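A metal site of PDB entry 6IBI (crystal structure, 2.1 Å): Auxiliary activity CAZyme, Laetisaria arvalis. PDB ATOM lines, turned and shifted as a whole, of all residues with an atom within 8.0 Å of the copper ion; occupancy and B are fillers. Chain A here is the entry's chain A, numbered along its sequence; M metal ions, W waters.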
ATOM      1  N   HIS A   1      14.159  19.175 -23.048  1.00  0.00           N
ATOM      2  CA  HIS A   1      13.765  17.754 -22.690  1.00  0.00           C
ATOM      3  C   HIS A   1      12.433  17.386 -23.341  1.00  0.00           C
ATOM      4  O   HIS A   1      11.744  18.243 -23.838  1.00  0.00           O
ATOM      5  CB  HIS A   1      13.700  17.616 -21.177  1.00  0.00           C
ATOM      6  CG  HIS A   1      15.050  17.664 -20.554  1.00  0.00           C
ATOM      7  ND1 HIS A   1      15.923  18.725 -20.744  1.00  0.00           N
ATOM      8  CD2 HIS A   1      15.671  16.766 -19.750  1.00  0.00           C
ATOM      9  CE1 HIS A   1      17.042  18.486 -20.087  1.00  0.00           C
ATOM     10  NE2 HIS A   1      16.903  17.269 -19.466  1.00  0.00           N
ATOM     11  N   PHE A   2      12.132  16.087 -23.426  1.00  0.00           N
ATOM     12  CA  PHE A   2      11.001  15.645 -24.254  1.00  0.00           C
ATOM     13  C   PHE A   2      10.398  14.349 -23.688  1.00  0.00           C
ATOM     14  O   PHE A   2      11.080  13.616 -23.006  1.00  0.00           O
ATOM     15  CB  PHE A   2      11.433  15.508 -25.701  1.00  0.00           C
ATOM     16  CG  PHE A   2      12.192  14.243 -26.016  1.00  0.00           C
ATOM     17  CD1 PHE A   2      13.548  14.145 -25.746  1.00  0.00           C
ATOM     18  CD2 PHE A   2      11.560  13.175 -26.604  1.00  0.00           C
ATOM     19  CE1 PHE A   2      14.239  12.975 -26.041  1.00  0.00           C
ATOM     20  CE2 PHE A   2      12.244  12.004 -26.894  1.00  0.00           C
ATOM     21  CZ  PHE A   2      13.598  11.922 -26.606  1.00  0.00           C
ATOM     22  N   ALA A  15      13.189  13.119 -16.303  1.00  0.00           N
ATOM     23  CA  ALA A  15      13.911  14.139 -17.085  1.00  0.00           C
ATOM     24  C   ALA A  15      15.423  14.007 -16.856  1.00  0.00           C
ATOM     25  O   ALA A  15      16.201  14.063 -17.796  1.00  0.00           O
ATOM     26  CB  ALA A  15      13.438  15.532 -16.705  1.00  0.00           C
ATOM     27  N   GLU A  18      17.387  11.357 -18.963  1.00  0.00           N
ATOM     28  CA  GLU A  18      17.315  11.356 -20.409  1.00  0.00           C
ATOM     29  C   GLU A  18      18.710  11.419 -21.018  1.00  0.00           C
ATOM     30  O   GLU A  18      18.873  11.182 -22.194  1.00  0.00           O
ATOM     31  CB  GLU A  18      16.439  12.497 -20.935  1.00  0.00           C
ATOM     32  CG  GLU A  18      14.963  12.243 -20.705  1.00  0.00           C
ATOM     33  CD  GLU A  18      14.042  12.999 -21.635  1.00  0.00           C
ATOM     34  OE1 GLU A  18      14.284  14.209 -21.867  1.00  0.00           O
ATOM     35  OE2 GLU A  18      13.101  12.371 -22.165  1.00  0.00           O
ATOM     36  N   SER A  47       8.217  18.339 -26.825  1.00  0.00           N
ATOM     37  CA  SER A  47       9.393  19.041 -26.313  1.00  0.00           C
ATOM     38  C   SER A  47       8.982  20.274 -25.480  1.00  0.00           C
ATOM     39  O   SER A  47       8.120  21.044 -25.850  1.00  0.00           O
ATOM     40  CB  SER A  47      10.273  19.468 -27.417  1.00  0.00           C
ATOM     41  OG  SER A  47      11.435  20.137 -26.930  1.00  0.00           O
ATOM     42  N   GLY A  48       9.627  20.413 -24.333  1.00  0.00           N
ATOM     43  CA  GLY A  48       9.494  21.546 -23.455  1.00  0.00           C
ATOM     44  C   GLY A  48      10.143  22.809 -23.994  1.00  0.00           C
ATOM     45  O   GLY A  48       9.819  23.862 -23.521  1.00  0.00           O
ATOM     46  N   HIS A  49      11.054  22.713 -24.951  1.00  0.00           N
ATOM     47  CA  HIS A  49      11.719  23.928 -25.488  1.00  0.00           C
ATOM     48  C   HIS A  49      12.205  23.715 -26.917  1.00  0.00           C
ATOM     49  O   HIS A  49      12.207  22.599 -27.427  1.00  0.00           O
ATOM     50  CB  HIS A  49      12.874  24.392 -24.584  1.00  0.00           C
ATOM     51  CG  HIS A  49      13.895  23.370 -24.223  1.00  0.00           C
ATOM     52  ND1 HIS A  49      15.048  23.191 -24.954  1.00  0.00           N
ATOM     53  CD2 HIS A  49      13.978  22.532 -23.150  1.00  0.00           C
ATOM     54  CE1 HIS A  49      15.808  22.278 -24.357  1.00  0.00           C
ATOM     55  NE2 HIS A  49      15.158  21.844 -23.252  1.00  0.00           N
ATOM     56  N   ALA A  50      12.575  24.822 -27.548  1.00  0.00           N
ATOM     57  CA  ALA A  50      12.952  24.860 -28.948  1.00  0.00           C
ATOM     58  C   ALA A  50      13.830  26.090 -29.163  1.00  0.00           C
ATOM     59  O   ALA A  50      13.735  27.050 -28.413  1.00  0.00           O
ATOM     60  CB  ALA A  50      11.731  24.895 -29.836  1.00  0.00           C
ATOM     61  N   TYR A  52      15.386  22.643 -31.327  1.00  0.00           N
ATOM     62  CA  TYR A  52      16.133  21.435 -31.021  1.00  0.00           C
ATOM     63  C   TYR A  52      16.324  20.634 -32.311  1.00  0.00           C
ATOM     64  O   TYR A  52      15.553  20.819 -33.249  1.00  0.00           O
ATOM     65  CB  TYR A  52      15.400  20.636 -29.921  1.00  0.00           C
ATOM     66  CG  TYR A  52      14.025  20.099 -30.278  1.00  0.00           C
ATOM     67  CD1 TYR A  52      12.885  20.848 -30.091  1.00  0.00           C
ATOM     68  CD2 TYR A  52      13.861  18.818 -30.805  1.00  0.00           C
ATOM     69  CE1 TYR A  52      11.623  20.367 -30.380  1.00  0.00           C
ATOM     70  CE2 TYR A  52      12.608  18.321 -31.118  1.00  0.00           C
ATOM     71  CZ  TYR A  52      11.480  19.086 -30.894  1.00  0.00           C
ATOM     72  OH  TYR A  52      10.214  18.608 -31.170  1.00  0.00           O
ATOM     73  N   TYR A 118      17.697  13.448 -29.217  1.00  0.00           N
ATOM     74  CA  TYR A 118      17.274  14.841 -29.088  1.00  0.00           C
ATOM     75  C   TYR A 118      18.459  15.675 -28.584  1.00  0.00           C
ATOM     76  O   TYR A 118      19.118  15.300 -27.621  1.00  0.00           O
ATOM     77  CB  TYR A 118      16.098  14.906 -28.116  1.00  0.00           C
ATOM     78  CG  TYR A 118      15.609  16.271 -27.674  1.00  0.00           C
ATOM     79  CD1 TYR A 118      16.301  17.044 -26.741  1.00  0.00           C
ATOM     80  CD2 TYR A 118      14.376  16.718 -28.097  1.00  0.00           C
ATOM     81  CE1 TYR A 118      15.818  18.266 -26.307  1.00  0.00           C
ATOM     82  CE2 TYR A 118      13.900  17.956 -27.687  1.00  0.00           C
ATOM     83  CZ  TYR A 118      14.621  18.739 -26.817  1.00  0.00           C
ATOM     84  OH  TYR A 118      14.063  19.908 -26.411  1.00  0.00           O
ATOM     85  N   THR A 119      18.688  16.807 -29.243  1.00  0.00           N
ATOM     86  CA  THR A 119      19.655  17.793 -28.811  1.00  0.00           C
ATOM     87  C   THR A 119      19.010  19.179 -28.834  1.00  0.00           C
ATOM     88  O   THR A 119      18.649  19.670 -29.915  1.00  0.00           O
ATOM     89  CB  THR A 119      20.814  17.747 -29.807  1.00  0.00           C
ATOM     90  OG1 THR A 119      21.524  16.544 -29.519  1.00  0.00           O
ATOM     91  CG2 THR A 119      21.761  18.919 -29.726  1.00  0.00           C
ATOM     92  N   GLY A 120      18.853  19.789 -27.660  1.00  0.00           N
ATOM     93  CA  GLY A 120      18.235  21.102 -27.561  1.00  0.00           C
ATOM     94  C   GLY A 120      19.067  22.055 -26.705  1.00  0.00           C
ATOM     95  O   GLY A 120      18.536  22.994 -26.159  1.00  0.00           O
ATOM     96  N   GLY A 121      20.365  21.789 -26.596  1.00  0.00           N
ATOM     97  CA  GLY A 121      21.289  22.685 -25.897  1.00  0.00           C
ATOM     98  C   GLY A 121      21.509  22.343 -24.432  1.00  0.00           C
ATOM     99  O   GLY A 121      22.391  22.927 -23.816  1.00  0.00           O
ATOM    100  N   ASP A 122      20.710  21.428 -23.862  1.00  0.00           N
ATOM    101  CA  ASP A 122      20.893  20.987 -22.465  1.00  0.00           C
ATOM    102  C   ASP A 122      21.251  19.485 -22.471  1.00  0.00           C
ATOM    103  O   ASP A 122      20.756  18.722 -21.642  1.00  0.00           O
ATOM    104  CB  ASP A 122      19.678  21.338 -21.589  1.00  0.00           C
ATOM    105  CG  ASP A 122      18.343  20.828 -22.100  1.00  0.00           C
ATOM    106  OD1 ASP A 122      18.330  20.207 -23.188  1.00  0.00           O
ATOM    107  OD2 ASP A 122      17.329  21.052 -21.427  1.00  0.00           O
ATOM    108  N   GLY A 123      22.108  19.075 -23.402  1.00  0.00           N
ATOM    109  CA  GLY A 123      22.616  17.716 -23.473  1.00  0.00           C
ATOM    110  C   GLY A 123      22.035  16.906 -24.623  1.00  0.00           C
ATOM    111  O   GLY A 123      21.121  17.355 -25.362  1.00  0.00           O
ATOM    112  N   LEU A 125      19.885  13.758 -25.408  1.00  0.00           N
ATOM    113  CA  LEU A 125      18.793  13.169 -24.642  1.00  0.00           C
ATOM    114  C   LEU A 125      18.139  12.049 -25.433  1.00  0.00           C
ATOM    115  O   LEU A 125      18.102  12.096 -26.694  1.00  0.00           O
ATOM    116  CB  LEU A 125      17.768  14.266 -24.331  1.00  0.00           C
ATOM    117  CG  LEU A 125      18.333  15.485 -23.625  1.00  0.00           C
ATOM    118  CD1 LEU A 125      17.209  16.449 -23.262  1.00  0.00           C
ATOM    119  CD2 LEU A 125      19.088  15.083 -22.361  1.00  0.00           C
HETATM  120 CU    CU M   1      15.659  20.199 -22.119  1.00  0.00          CU
HETATM  121  O   HOH W   1      14.533  20.932 -20.016  1.00  0.00           O
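The copper ion is bound by the side-chain carboxylate of Asp 122, a ring nitrogen (ND1) of His 1, the backbone nitrogen of His 1, a ring nitrogen (NE2) of His 49 and water W1.
The nearest printed residue that does not touch the copper ion is Leu 125 (4.2 Å).
N of His 1 sits close to OH of Tyr 118 (3.4 Å).
O of His 1 sits at hydrogen-bond distance from N of Gly 48 (3.1 Å).
The side-chain hydroxyl (OH) of Tyr 118 is in hydrogen-bond range of the backbone carbonyl oxygen (O) of His 49 (3.4 Å).
OG of Ser 47 lies within hydrogen-bond range of O of His 49, at 2.6 Å.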
